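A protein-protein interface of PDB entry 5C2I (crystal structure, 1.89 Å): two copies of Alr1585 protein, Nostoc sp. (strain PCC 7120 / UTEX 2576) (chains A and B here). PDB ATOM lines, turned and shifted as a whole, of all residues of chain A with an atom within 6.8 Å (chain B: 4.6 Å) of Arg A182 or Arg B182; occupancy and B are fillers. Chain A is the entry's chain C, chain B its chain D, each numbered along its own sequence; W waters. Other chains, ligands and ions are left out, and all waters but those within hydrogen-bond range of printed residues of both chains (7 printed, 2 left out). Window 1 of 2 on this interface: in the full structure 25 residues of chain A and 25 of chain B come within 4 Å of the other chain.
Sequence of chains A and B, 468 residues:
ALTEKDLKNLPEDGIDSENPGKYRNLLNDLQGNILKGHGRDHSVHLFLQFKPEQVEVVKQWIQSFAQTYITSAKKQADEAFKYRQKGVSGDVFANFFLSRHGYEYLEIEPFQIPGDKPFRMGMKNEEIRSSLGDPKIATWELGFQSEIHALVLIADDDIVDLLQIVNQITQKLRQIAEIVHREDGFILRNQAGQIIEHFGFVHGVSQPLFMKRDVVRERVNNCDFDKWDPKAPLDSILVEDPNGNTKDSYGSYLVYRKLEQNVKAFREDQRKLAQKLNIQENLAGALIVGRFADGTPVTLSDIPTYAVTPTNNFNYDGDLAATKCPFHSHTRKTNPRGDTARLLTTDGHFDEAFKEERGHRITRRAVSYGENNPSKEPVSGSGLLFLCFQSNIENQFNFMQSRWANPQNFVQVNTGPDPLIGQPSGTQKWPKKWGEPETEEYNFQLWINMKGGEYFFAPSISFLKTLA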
ATOM      1  N   SER A  43      13.745 -31.491  30.570  1.00  0.00           N
ATOM      2  CA  SER A  43      13.619 -30.788  29.330  1.00  0.00           C
ATOM      3  C   SER A  43      13.588 -29.280  29.535  1.00  0.00           C
ATOM      4  O   SER A  43      13.321 -28.798  30.634  1.00  0.00           O
ATOM      5  CB  SER A  43      12.380 -31.279  28.577  1.00  0.00           C
ATOM      6  OG  SER A  43      11.253 -30.966  29.312  1.00  0.00           O
ATOM      7  N   VAL A  44      13.913 -28.576  28.454  1.00  0.00           N
ATOM      8  CA  VAL A  44      13.829 -27.147  28.390  1.00  0.00           C
ATOM      9  C   VAL A  44      12.971 -26.793  27.210  1.00  0.00           C
ATOM     10  O   VAL A  44      13.139 -27.320  26.099  1.00  0.00           O
ATOM     11  CB  VAL A  44      15.224 -26.474  28.298  1.00  0.00           C
ATOM     12  CG1 VAL A  44      15.086 -24.947  28.159  1.00  0.00           C
ATOM     13  CG2 VAL A  44      16.087 -26.825  29.507  1.00  0.00           C
ATOM     14  N   HIS A  45      12.003 -25.924  27.466  1.00  0.00           N
ATOM     15  CA  HIS A  45      11.103 -25.409  26.452  1.00  0.00           C
ATOM     16  C   HIS A  45      11.361 -23.906  26.281  1.00  0.00           C
ATOM     17  O   HIS A  45      11.211 -23.148  27.233  1.00  0.00           O
ATOM     18  CB  HIS A  45       9.672 -25.596  26.903  1.00  0.00           C
ATOM     19  CG  HIS A  45       9.272 -27.023  27.104  1.00  0.00           C
ATOM     20  ND1 HIS A  45       8.107 -27.370  27.744  1.00  0.00           N
ATOM     21  CD2 HIS A  45       9.853 -28.181  26.732  1.00  0.00           C
ATOM     22  CE1 HIS A  45       7.994 -28.677  27.783  1.00  0.00           C
ATOM     23  NE2 HIS A  45       9.054 -29.196  27.196  1.00  0.00           N
ATOM     24  N   LEU A  46      11.780 -23.503  25.077  1.00  0.00           N
ATOM     25  CA  LEU A  46      12.052 -22.101  24.759  1.00  0.00           C
ATOM     26  C   LEU A  46      11.073 -21.606  23.722  1.00  0.00           C
ATOM     27  O   LEU A  46      11.049 -22.101  22.584  1.00  0.00           O
ATOM     28  CB  LEU A  46      13.475 -21.912  24.230  1.00  0.00           C
ATOM     29  CG  LEU A  46      14.624 -22.419  25.095  1.00  0.00           C
ATOM     30  CD1 LEU A  46      15.960 -22.270  24.352  1.00  0.00           C
ATOM     31  CD2 LEU A  46      14.653 -21.717  26.434  1.00  0.00           C
ATOM     32  N   PHE A  47      10.251 -20.633  24.125  1.00  0.00           N
ATOM     33  CA  PHE A  47       9.270 -20.045  23.243  1.00  0.00           C
ATOM     34  C   PHE A  47       9.840 -18.800  22.625  1.00  0.00           C
ATOM     35  O   PHE A  47      10.358 -17.938  23.321  1.00  0.00           O
ATOM     36  CB  PHE A  47       7.999 -19.716  24.006  1.00  0.00           C
ATOM     37  CG  PHE A  47       7.250 -20.933  24.471  1.00  0.00           C
ATOM     38  CD1 PHE A  47       7.535 -21.542  25.671  1.00  0.00           C
ATOM     39  CD2 PHE A  47       6.272 -21.475  23.669  1.00  0.00           C
ATOM     40  CE1 PHE A  47       6.841 -22.683  26.079  1.00  0.00           C
ATOM     41  CE2 PHE A  47       5.568 -22.602  24.056  1.00  0.00           C
ATOM     42  CZ  PHE A  47       5.840 -23.201  25.262  1.00  0.00           C
ATOM     43  N   GLY A 143       4.416 -14.538  29.558  1.00  0.00           N
ATOM     44  CA  GLY A 143       5.151 -15.162  28.448  1.00  0.00           C
ATOM     45  C   GLY A 143       4.266 -15.650  27.317  1.00  0.00           C
ATOM     46  O   GLY A 143       4.577 -15.452  26.122  1.00  0.00           O
ATOM     47  N   ILE A 159      20.751 -33.272  33.883  1.00  0.00           N
ATOM     48  CA  ILE A 159      20.229 -31.885  33.965  1.00  0.00           C
ATOM     49  C   ILE A 159      21.355 -30.836  33.827  1.00  0.00           C
ATOM     50  O   ILE A 159      21.217 -29.888  33.055  1.00  0.00           O
ATOM     51  CB  ILE A 159      19.368 -31.658  35.231  1.00  0.00           C
ATOM     52  CG1 ILE A 159      18.757 -30.255  35.258  1.00  0.00           C
ATOM     53  CG2 ILE A 159      20.161 -31.851  36.510  1.00  0.00           C
ATOM     54  CD1 ILE A 159      17.963 -29.877  34.031  1.00  0.00           C
ATOM     55  N   LEU A 162      22.396 -30.617  30.205  1.00  0.00           N
ATOM     56  CA  LEU A 162      21.306 -30.008  29.456  1.00  0.00           C
ATOM     57  C   LEU A 162      21.348 -28.477  29.560  1.00  0.00           C
ATOM     58  O   LEU A 162      21.181 -27.771  28.558  1.00  0.00           O
ATOM     59  CB  LEU A 162      19.960 -30.506  29.957  1.00  0.00           C
ATOM     60  CG  LEU A 162      18.696 -29.891  29.386  1.00  0.00           C
ATOM     61  CD1 LEU A 162      18.626 -30.051  27.873  1.00  0.00           C
ATOM     62  CD2 LEU A 162      17.434 -30.457  30.041  1.00  0.00           C
ATOM     63  N   LEU A 163      21.541 -27.975  30.768  1.00  0.00           N
ATOM     64  CA  LEU A 163      21.570 -26.528  30.975  1.00  0.00           C
ATOM     65  C   LEU A 163      22.736 -25.858  30.233  1.00  0.00           C
ATOM     66  O   LEU A 163      22.565 -24.781  29.639  1.00  0.00           O
ATOM     67  CB  LEU A 163      21.663 -26.208  32.462  1.00  0.00           C
ATOM     68  CG  LEU A 163      20.492 -26.732  33.300  1.00  0.00           C
ATOM     69  CD1 LEU A 163      20.786 -26.545  34.786  1.00  0.00           C
ATOM     70  CD2 LEU A 163      19.181 -26.052  32.935  1.00  0.00           C
ATOM     71  N   VAL A 166      21.918 -25.878  26.455  1.00  0.00           N
ATOM     72  CA  VAL A 166      20.931 -24.828  26.219  1.00  0.00           C
ATOM     73  C   VAL A 166      21.582 -23.445  26.215  1.00  0.00           C
ATOM     74  O   VAL A 166      21.321 -22.651  25.294  1.00  0.00           O
ATOM     75  CB  VAL A 166      19.763 -24.906  27.202  1.00  0.00           C
ATOM     76  CG1 VAL A 166      18.921 -23.643  27.123  1.00  0.00           C
ATOM     77  CG2 VAL A 166      18.900 -26.122  26.875  1.00  0.00           C
ATOM     78  N   ASN A 167      22.456 -23.160  27.188  1.00  0.00           N
ATOM     79  CA  ASN A 167      23.098 -21.848  27.230  1.00  0.00           C
ATOM     80  C   ASN A 167      23.996 -21.599  26.033  1.00  0.00           C
ATOM     81  O   ASN A 167      24.107 -20.463  25.562  1.00  0.00           O
ATOM     82  CB  ASN A 167      23.879 -21.669  28.516  1.00  0.00           C
ATOM     83  CG  ASN A 167      22.971 -21.557  29.718  1.00  0.00           C
ATOM     84  OD1 ASN A 167      21.787 -21.246  29.580  1.00  0.00           O
ATOM     85  ND2 ASN A 167      23.508 -21.840  30.897  1.00  0.00           N
ATOM     86  N   GLN A 168      24.592 -22.660  25.509  1.00  0.00           N
ATOM     87  CA  GLN A 168      25.368 -22.542  24.272  1.00  0.00           C
ATOM     88  C   GLN A 168      24.451 -22.239  23.086  1.00  0.00           C
ATOM     89  O   GLN A 168      24.698 -21.317  22.336  1.00  0.00           O
ATOM     90  CB  GLN A 168      26.142 -23.836  24.020  1.00  0.00           C
ATOM     91  CG  GLN A 168      27.077 -23.783  22.841  1.00  0.00           C
ATOM     92  CD  GLN A 168      27.968 -25.032  22.778  1.00  0.00           C
ATOM     93  OE1 GLN A 168      28.124 -25.769  23.757  1.00  0.00           O
ATOM     94  NE2 GLN A 168      28.525 -25.278  21.622  1.00  0.00           N
ATOM     95  N   THR A 170      21.540 -20.911  22.996  1.00  0.00           N
ATOM     96  CA  THR A 170      20.866 -19.631  23.066  1.00  0.00           C
ATOM     97  C   THR A 170      21.732 -18.414  22.713  1.00  0.00           C
ATOM     98  O   THR A 170      21.191 -17.352  22.431  1.00  0.00           O
ATOM     99  CB  THR A 170      20.171 -19.398  24.421  1.00  0.00           C
ATOM    100  OG1 THR A 170      21.113 -19.485  25.478  1.00  0.00           O
ATOM    101  CG2 THR A 170      19.091 -20.434  24.628  1.00  0.00           C
ATOM    102  N   GLN A 171      23.046 -18.562  22.664  1.00  0.00           N
ATOM    103  CA  GLN A 171      23.896 -17.435  22.291  1.00  0.00           C
ATOM    104  C   GLN A 171      23.606 -16.935  20.893  1.00  0.00           C
ATOM    105  O   GLN A 171      23.392 -15.753  20.712  1.00  0.00           O
ATOM    106  CB  GLN A 171      25.371 -17.768  22.425  1.00  0.00           C
ATOM    107  CG  GLN A 171      25.771 -17.966  23.876  1.00  0.00           C
ATOM    108  CD  GLN A 171      27.138 -17.421  24.178  1.00  0.00           C
ATOM    109  OE1 GLN A 171      27.438 -16.268  23.897  1.00  0.00           O
ATOM    110  NE2 GLN A 171      27.965 -18.241  24.803  1.00  0.00           N
ATOM    111  N   ARG A 174      19.667 -15.844  20.452  1.00  0.00           N
ATOM    112  CA  ARG A 174      19.260 -14.511  20.936  1.00  0.00           C
ATOM    113  C   ARG A 174      19.543 -13.413  19.933  1.00  0.00           C
ATOM    114  O   ARG A 174      18.939 -12.357  19.999  1.00  0.00           O
ATOM    115  CB  ARG A 174      19.973 -14.161  22.238  1.00  0.00           C
ATOM    116  CG  ARG A 174      19.406 -14.868  23.455  1.00  0.00           C
ATOM    117  CD  ARG A 174      20.138 -14.461  24.733  1.00  0.00           C
ATOM    118  NE  ARG A 174      19.593 -15.237  25.840  1.00  0.00           N
ATOM    119  CZ  ARG A 174      20.225 -16.191  26.527  1.00  0.00           C
ATOM    120  NH1 ARG A 174      21.521 -16.504  26.296  1.00  0.00           N
ATOM    121  NH2 ARG A 174      19.529 -16.832  27.484  1.00  0.00           N
ATOM    122  N   ILE A 179      13.507 -14.729  23.315  1.00  0.00           N
ATOM    123  CA  ILE A 179      12.990 -15.851  24.065  1.00  0.00           C
ATOM    124  C   ILE A 179      11.925 -15.257  24.986  1.00  0.00           C
ATOM    125  O   ILE A 179      12.257 -14.586  25.947  1.00  0.00           O
ATOM    126  CB  ILE A 179      14.103 -16.542  24.855  1.00  0.00           C
ATOM    127  CG1 ILE A 179      15.125 -17.137  23.881  1.00  0.00           C
ATOM    128  CG2 ILE A 179      13.512 -17.626  25.745  1.00  0.00           C
ATOM    129  CD1 ILE A 179      16.388 -17.657  24.523  1.00  0.00           C
ATOM    130  N   VAL A 180      10.652 -15.459  24.656  1.00  0.00           N
ATOM    131  CA  VAL A 180       9.567 -14.771  25.352  1.00  0.00           C
ATOM    132  C   VAL A 180       9.124 -15.549  26.585  1.00  0.00           C
ATOM    133  O   VAL A 180       8.466 -15.009  27.468  1.00  0.00           O
ATOM    134  CB  VAL A 180       8.368 -14.432  24.421  1.00  0.00           C
ATOM    135  CG1 VAL A 180       8.815 -13.543  23.274  1.00  0.00           C
ATOM    136  CG2 VAL A 180       7.674 -15.699  23.891  1.00  0.00           C
ATOM    137  N   HIS A 181       9.478 -16.830  26.652  1.00  0.00           N
ATOM    138  CA  HIS A 181       9.084 -17.690  27.757  1.00  0.00           C
ATOM    139  C   HIS A 181       9.946 -18.958  27.793  1.00  0.00           C
ATOM    140  O   HIS A 181      10.390 -19.447  26.750  1.00  0.00           O
ATOM    141  CB  HIS A 181       7.617 -18.105  27.632  1.00  0.00           C
ATOM    142  CG  HIS A 181       7.099 -18.790  28.840  1.00  0.00           C
ATOM    143  ND1 HIS A 181       7.047 -18.168  30.070  1.00  0.00           N
ATOM    144  CD2 HIS A 181       6.732 -20.074  29.052  1.00  0.00           C
ATOM    145  CE1 HIS A 181       6.604 -19.020  30.969  1.00  0.00           C
ATOM    146  NE2 HIS A 181       6.408 -20.181  30.380  1.00  0.00           N
ATOM    147  N   ARG A 182      10.217 -19.429  28.998  1.00  0.00           N
ATOM    148  CA  ARG A 182      10.973 -20.669  29.218  1.00  0.00           C
ATOM    149  C   ARG A 182      10.301 -21.523  30.280  1.00  0.00           C
ATOM    150  O   ARG A 182       9.817 -21.023  31.292  1.00  0.00           O
ATOM    151  CB  ARG A 182      12.424 -20.364  29.643  1.00  0.00           C
ATOM    152  CG  ARG A 182      13.237 -21.613  30.003  1.00  0.00           C
ATOM    153  CD  ARG A 182      14.693 -21.316  30.300  1.00  0.00           C
ATOM    154  NE  ARG A 182      15.375 -22.480  30.876  1.00  0.00           N
ATOM    155  CZ  ARG A 182      16.677 -22.727  30.826  1.00  0.00           C
ATOM    156  NH1 ARG A 182      17.499 -21.920  30.166  1.00  0.00           N
ATOM    157  NH2 ARG A 182      17.156 -23.826  31.398  1.00  0.00           N
ATOM    158  N   GLU A 183      10.337 -22.823  30.058  1.00  0.00           N
ATOM    159  CA  GLU A 183      10.014 -23.807  31.077  1.00  0.00           C
ATOM    160  C   GLU A 183      11.124 -24.828  31.158  1.00  0.00           C
ATOM    161  O   GLU A 183      11.860 -25.088  30.194  1.00  0.00           O
ATOM    162  CB  GLU A 183       8.688 -24.540  30.774  1.00  0.00           C
ATOM    163  CG  GLU A 183       7.451 -23.668  30.732  1.00  0.00           C
ATOM    164  CD  GLU A 183       6.998 -23.149  32.089  1.00  0.00           C
ATOM    165  OE1 GLU A 183       7.434 -23.661  33.156  1.00  0.00           O
ATOM    166  OE2 GLU A 183       6.174 -22.207  32.106  1.00  0.00           O
ATOM    167  N   ASP A 184      11.270 -25.383  32.350  1.00  0.00           N
ATOM    168  CA  ASP A 184      12.207 -26.471  32.631  1.00  0.00           C
ATOM    169  C   ASP A 184      11.366 -27.613  33.164  1.00  0.00           C
ATOM    170  O   ASP A 184      11.051 -27.664  34.363  1.00  0.00           O
ATOM    171  CB  ASP A 184      13.242 -26.040  33.663  1.00  0.00           C
ATOM    172  CG  ASP A 184      14.316 -25.152  33.068  1.00  0.00           C
ATOM    173  OD1 ASP A 184      14.085 -23.914  32.965  1.00  0.00           O
ATOM    174  OD2 ASP A 184      15.385 -25.707  32.699  1.00  0.00           O
ATOM    175  N   TYR A 256       0.048 -27.357  23.149  1.00  0.00           N
ATOM    176  CA  TYR A 256       0.827 -27.073  24.361  1.00  0.00           C
ATOM    177  C   TYR A 256      -0.020 -26.197  25.275  1.00  0.00           C
ATOM    178  O   TYR A 256      -0.480 -25.163  24.842  1.00  0.00           O
ATOM    179  CB  TYR A 256       2.114 -26.310  24.008  1.00  0.00           C
ATOM    180  CG  TYR A 256       3.117 -26.184  25.135  1.00  0.00           C
ATOM    181  CD1 TYR A 256       2.846 -25.439  26.282  1.00  0.00           C
ATOM    182  CD2 TYR A 256       4.345 -26.801  25.046  1.00  0.00           C
ATOM    183  CE1 TYR A 256       3.772 -25.325  27.303  1.00  0.00           C
ATOM    184  CE2 TYR A 256       5.288 -26.709  26.080  1.00  0.00           C
ATOM    185  CZ  TYR A 256       4.988 -25.975  27.201  1.00  0.00           C
ATOM    186  OH  TYR A 256       5.908 -25.895  28.200  1.00  0.00           O
ATOM    187  N   LYS A 258      -0.132 -24.900  29.483  1.00  0.00           N
ATOM    188  CA  LYS A 258       0.388 -24.885  30.839  1.00  0.00           C
ATOM    189  C   LYS A 258      -0.793 -24.931  31.810  1.00  0.00           C
ATOM    190  O   LYS A 258      -1.590 -24.003  31.857  1.00  0.00           O
ATOM    191  CB  LYS A 258       1.253 -23.651  31.105  1.00  0.00           C
ATOM    192  CG  LYS A 258       1.831 -23.593  32.512  1.00  0.00           C
ATOM    193  CD  LYS A 258       2.865 -22.456  32.668  1.00  0.00           C
ATOM    194  CE  LYS A 258       3.538 -22.539  34.049  1.00  0.00           C
ATOM    195  NZ  LYS A 258       4.613 -21.526  34.226  1.00  0.00           N
ATOM    196  N   VAL B  44      22.349 -19.668  38.931  1.00  0.00           N
ATOM    197  CA  VAL B  44      21.960 -19.109  37.651  1.00  0.00           C
ATOM    198  C   VAL B  44      22.410 -17.649  37.647  1.00  0.00           C
ATOM    199  O   VAL B  44      22.170 -16.897  38.600  1.00  0.00           O
ATOM    200  CB  VAL B  44      20.448 -19.212  37.390  1.00  0.00           C
ATOM    201  CG1 VAL B  44      20.070 -18.523  36.073  1.00  0.00           C
ATOM    202  CG2 VAL B  44      19.996 -20.663  37.374  1.00  0.00           C
ATOM    203  N   HIS B  45      23.074 -17.286  36.567  1.00  0.00           N
ATOM    204  CA  HIS B  45      23.533 -15.934  36.349  1.00  0.00           C
ATOM    205  C   HIS B  45      22.795 -15.369  35.149  1.00  0.00           C
ATOM    206  O   HIS B  45      22.923 -15.900  34.053  1.00  0.00           O
ATOM    207  CB  HIS B  45      25.015 -15.926  36.042  1.00  0.00           C
ATOM    208  CG  HIS B  45      25.870 -16.455  37.138  1.00  0.00           C
ATOM    209  ND1 HIS B  45      27.192 -16.798  36.940  1.00  0.00           N
ATOM    210  CD2 HIS B  45      25.615 -16.688  38.439  1.00  0.00           C
ATOM    211  CE1 HIS B  45      27.709 -17.202  38.080  1.00  0.00           C
ATOM    212  NE2 HIS B  45      26.778 -17.119  39.007  1.00  0.00           N
ATOM    213  N   LEU B  46      22.039 -14.293  35.364  1.00  0.00           N
ATOM    214  CA  LEU B  46      21.299 -13.611  34.304  1.00  0.00           C
ATOM    215  C   LEU B  46      21.866 -12.218  34.110  1.00  0.00           C
ATOM    216  O   LEU B  46      21.788 -11.361  35.001  1.00  0.00           O
ATOM    217  CB  LEU B  46      19.823 -13.518  34.645  1.00  0.00           C
ATOM    218  CG  LEU B  46      19.082 -14.816  34.992  1.00  0.00           C
ATOM    219  CD1 LEU B  46      17.660 -14.499  35.432  1.00  0.00           C
ATOM    220  CD2 LEU B  46      19.124 -15.787  33.833  1.00  0.00           C
ATOM    221  N   LEU B 163      15.554 -23.891  38.997  1.00  0.00           N
ATOM    222  CA  LEU B 163      15.126 -23.594  37.618  1.00  0.00           C
ATOM    223  C   LEU B 163      13.720 -23.043  37.606  1.00  0.00           C
ATOM    224  O   LEU B 163      13.405 -22.109  36.832  1.00  0.00           O
ATOM    225  CB  LEU B 163      15.226 -24.830  36.739  1.00  0.00           C
ATOM    226  CG  LEU B 163      16.638 -25.377  36.601  1.00  0.00           C
ATOM    227  CD1 LEU B 163      16.624 -26.735  35.885  1.00  0.00           C
ATOM    228  CD2 LEU B 163      17.585 -24.419  35.899  1.00  0.00           C
ATOM    229  N   VAL B 166      13.661 -19.426  38.986  1.00  0.00           N
ATOM    230  CA  VAL B 166      14.197 -18.545  37.970  1.00  0.00           C
ATOM    231  C   VAL B 166      13.164 -18.283  36.872  1.00  0.00           C
ATOM    232  O   VAL B 166      12.975 -17.136  36.453  1.00  0.00           O
ATOM    233  CB  VAL B 166      15.515 -19.084  37.384  1.00  0.00           C
ATOM    234  CG1 VAL B 166      15.891 -18.340  36.122  1.00  0.00           C
ATOM    235  CG2 VAL B 166      16.620 -18.957  38.399  1.00  0.00           C
ATOM    236  N   ASN B 167      12.490 -19.323  36.392  1.00  0.00           N
ATOM    237  CA  ASN B 167      11.506 -19.126  35.317  1.00  0.00           C
ATOM    238  C   ASN B 167      10.368 -18.231  35.782  1.00  0.00           C
ATOM    239  O   ASN B 167       9.805 -17.477  34.984  1.00  0.00           O
ATOM    240  CB  ASN B 167      10.975 -20.459  34.803  1.00  0.00           C
ATOM    241  CG  ASN B 167      12.033 -21.224  34.034  1.00  0.00           C
ATOM    242  OD1 ASN B 167      13.011 -20.635  33.560  1.00  0.00           O
ATOM    243  ND2 ASN B 167      11.854 -22.516  33.908  1.00  0.00           N
ATOM    244  N   ARG B 174      11.394 -10.011  32.050  1.00  0.00           N
ATOM    245  CA  ARG B 174      11.454  -9.862  30.597  1.00  0.00           C
ATOM    246  C   ARG B 174      10.654  -8.664  30.079  1.00  0.00           C
ATOM    247  O   ARG B 174      10.901  -8.194  28.990  1.00  0.00           O
ATOM    248  CB  ARG B 174      10.945 -11.122  29.893  1.00  0.00           C
ATOM    249  CG  ARG B 174      11.952 -12.260  29.900  1.00  0.00           C
ATOM    250  CD  ARG B 174      11.414 -13.495  29.164  1.00  0.00           C
ATOM    251  NE  ARG B 174      12.394 -14.574  29.272  1.00  0.00           N
ATOM    252  CZ  ARG B 174      12.260 -15.698  29.973  1.00  0.00           C
ATOM    253  NH1 ARG B 174      11.107 -16.011  30.625  1.00  0.00           N
ATOM    254  NH2 ARG B 174      13.310 -16.537  30.003  1.00  0.00           N
ATOM    255  N   HIS B 181      22.427 -12.702  28.362  1.00  0.00           N
ATOM    256  CA  HIS B 181      23.268 -13.860  28.577  1.00  0.00           C
ATOM    257  C   HIS B 181      22.880 -14.593  29.845  1.00  0.00           C
ATOM    258  O   HIS B 181      22.427 -13.956  30.813  1.00  0.00           O
ATOM    259  CB  HIS B 181      24.743 -13.448  28.691  1.00  0.00           C
ATOM    260  CG  HIS B 181      25.674 -14.617  28.717  1.00  0.00           C
ATOM    261  ND1 HIS B 181      25.776 -15.498  27.667  1.00  0.00           N
ATOM    262  CD2 HIS B 181      26.491 -15.088  29.684  1.00  0.00           C
ATOM    263  CE1 HIS B 181      26.652 -16.438  27.959  1.00  0.00           C
ATOM    264  NE2 HIS B 181      27.090 -16.225  29.187  1.00  0.00           N
ATOM    265  N   ARG B 182      23.040 -15.922  29.822  1.00  0.00           N
ATOM    266  CA  ARG B 182      22.775 -16.768  30.980  1.00  0.00           C
ATOM    267  C   ARG B 182      23.863 -17.804  31.176  1.00  0.00           C
ATOM    268  O   ARG B 182      24.389 -18.386  30.214  1.00  0.00           O
ATOM    269  CB  ARG B 182      21.432 -17.492  30.829  1.00  0.00           C
ATOM    270  CG  ARG B 182      21.132 -18.471  31.954  1.00  0.00           C
ATOM    271  CD  ARG B 182      19.754 -19.095  31.881  1.00  0.00           C
ATOM    272  NE  ARG B 182      19.600 -20.226  32.813  1.00  0.00           N
ATOM    273  CZ  ARG B 182      18.447 -20.629  33.351  1.00  0.00           C
ATOM    274  NH1 ARG B 182      17.303 -19.984  33.109  1.00  0.00           N
ATOM    275  NH2 ARG B 182      18.436 -21.691  34.142  1.00  0.00           N
ATOM    276  N   GLU B 183      24.216 -18.030  32.441  1.00  0.00           N
ATOM    277  CA  GLU B 183      25.025 -19.179  32.833  1.00  0.00           C
ATOM    278  C   GLU B 183      24.296 -19.962  33.927  1.00  0.00           C
ATOM    279  O   GLU B 183      23.522 -19.406  34.707  1.00  0.00           O
ATOM    280  CB  GLU B 183      26.415 -18.758  33.340  1.00  0.00           C
ATOM    281  CG  GLU B 183      27.295 -18.030  32.321  1.00  0.00           C
ATOM    282  CD  GLU B 183      27.867 -18.923  31.220  1.00  0.00           C
ATOM    283  OE1 GLU B 183      27.825 -20.170  31.316  1.00  0.00           O
ATOM    284  OE2 GLU B 183      28.333 -18.339  30.216  1.00  0.00           O
ATOM    285  N   ASP B 184      24.581 -21.250  33.964  1.00  0.00           N
ATOM    286  CA  ASP B 184      24.103 -22.160  35.004  1.00  0.00           C
ATOM    287  C   ASP B 184      25.345 -22.766  35.635  1.00  0.00           C
ATOM    288  O   ASP B 184      25.936 -23.725  35.106  1.00  0.00           O
ATOM    289  CB  ASP B 184      23.231 -23.251  34.407  1.00  0.00           C
ATOM    290  CG  ASP B 184      21.846 -22.742  34.056  1.00  0.00           C
ATOM    291  OD1 ASP B 184      21.676 -22.139  32.964  1.00  0.00           O
ATOM    292  OD2 ASP B 184      20.942 -22.919  34.909  1.00  0.00           O
HETATM  293  O   HOH W   1      16.287 -16.613  28.732  1.00  0.00           O
HETATM  294  O   HOH W   2       8.192 -15.407  30.411  1.00  0.00           O
HETATM  295  O   HOH W   3       9.650 -24.418  34.507  1.00  0.00           O
HETATM  296  O   HOH W   4      23.531 -18.104  27.415  1.00  0.00           O
HETATM  297  O   HOH W   5      26.324 -22.390  31.915  1.00  0.00           O
HETATM  298  O   HOH W   6      24.042 -15.099  25.286  1.00  0.00           O
HETATM  299  O   HOH W   7      10.050 -18.321  32.169  1.00  0.00           O
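Hydrophobic or aromatic side chains of chain A that line the printed part of chain B: Ile A159 and Leu A163. Of the 11 printed residues of chain B, 7 touch a printed residue of chain A. Hydrophobic or aromatic side chains of chain B within 4 Å of the printed part of chain A: Leu B163 and His B181. Among the printed residues, 18 pairs touch across the chains. Among the printed residues, no Asp or Glu carboxylate lies within 4 Å of a Lys or Arg side-chain nitrogen of the other chain.
The backbone carbonyl oxygen (O) of Phe A47 lies within hydrogen-bond range of the backbone NH (N) of Val A180, at 2.8 Å. NE of Arg B182 lies within salt-bridge range of OD1 of Asp B184 (2.8 Å). NE2 of His B181 lies within hydrogen-bond range of OE2 of Glu B183 (2.7 Å).
Of chain A, only Asn A167 (3.5 Å), Arg A174 (3.9 Å) and Arg A182 (3.5 Å) come within 4 Å of Arg B182. Printed residues of chain B within 4 Å of Ile A159: Leu B163. Printed residues of chain B within 4 Å of Arg A174: His B181 (3.9 Å) and Arg B182 (3.9 Å). Of the printed residues of chain B, Ile A179 touches Arg B174 (3.3 Å). Printed residues of chain B within 4 Å of Asp A184: Leu B163 and Asn B167. Tyr A256 touches none of the printed residues of chain B. The nearest printed residue of chain B that does not touch Arg A182 is Leu B163 (4.6 Å). The nearest printed residue of chain B that does not touch Leu A163 is Arg B182 (4.6 Å).
OD1 of Asp B184 is in hydrogen-bond range of ND2 of Asn A167, 2.8 Å away. NE of Arg B174 is in hydrogen-bond range of O of Ile A179, at 3.3 Å. The side-chain amide nitrogen (ND2) of Asn B167 sits at hydrogen-bond distance from the side-chain carboxylate (OD1) of Asp A184 (2.8 Å).
Asn A167 touches Arg B182, and with the chains exchanged Arg A182 touches Asn B167. Asn A167 touches Glu B183, and with the chains exchanged Glu A183 touches Asn B167. 11 positions are printed for both chains. Of the 18 pairs that touch across the chains among the printed residues, 14 have their exchanged pair printed and touching as well.
Among the printed residues, merely in contact across the chains: Ile A159 with Leu B163 (3.9 Å), Leu A163 with Leu B163 (3.7 Å), Leu A163 with Asp B184 (3.6 Å), Asn A167 with Arg B182 (3.5 Å), Asn A167 with Glu B183 (3.6 Å), Gln A171 with His B181 (3.9 Å), Arg A174 with His B181 (3.9 Å), Arg A174 with Arg B182 (3.9 Å), Val A180 with Arg B174 (3.7 Å), His A181 with Arg B174 (3.9 Å), Arg A182 with Asn B167 (3.5 Å), Arg A182 with Arg B174 (3.9 Å), Arg A182 with Arg B182 (3.5 Å), Glu A183 with Asn B167 (3.6 Å) and Asp A184 with Leu B163 (3.6 Å).
Water W4 lies within hydrogen-bond range of the guanidinium group of Arg A174 (2.8 Å), the backbone carbonyl oxygen of Arg B182 (2.9 Å), the backbone carbonyl oxygen of Asn A167 (3.1 Å), the side-chain hydroxyl of Thr A170 (3.4 Å) and a ring nitrogen (ND1) of His B181 (3.4 Å).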
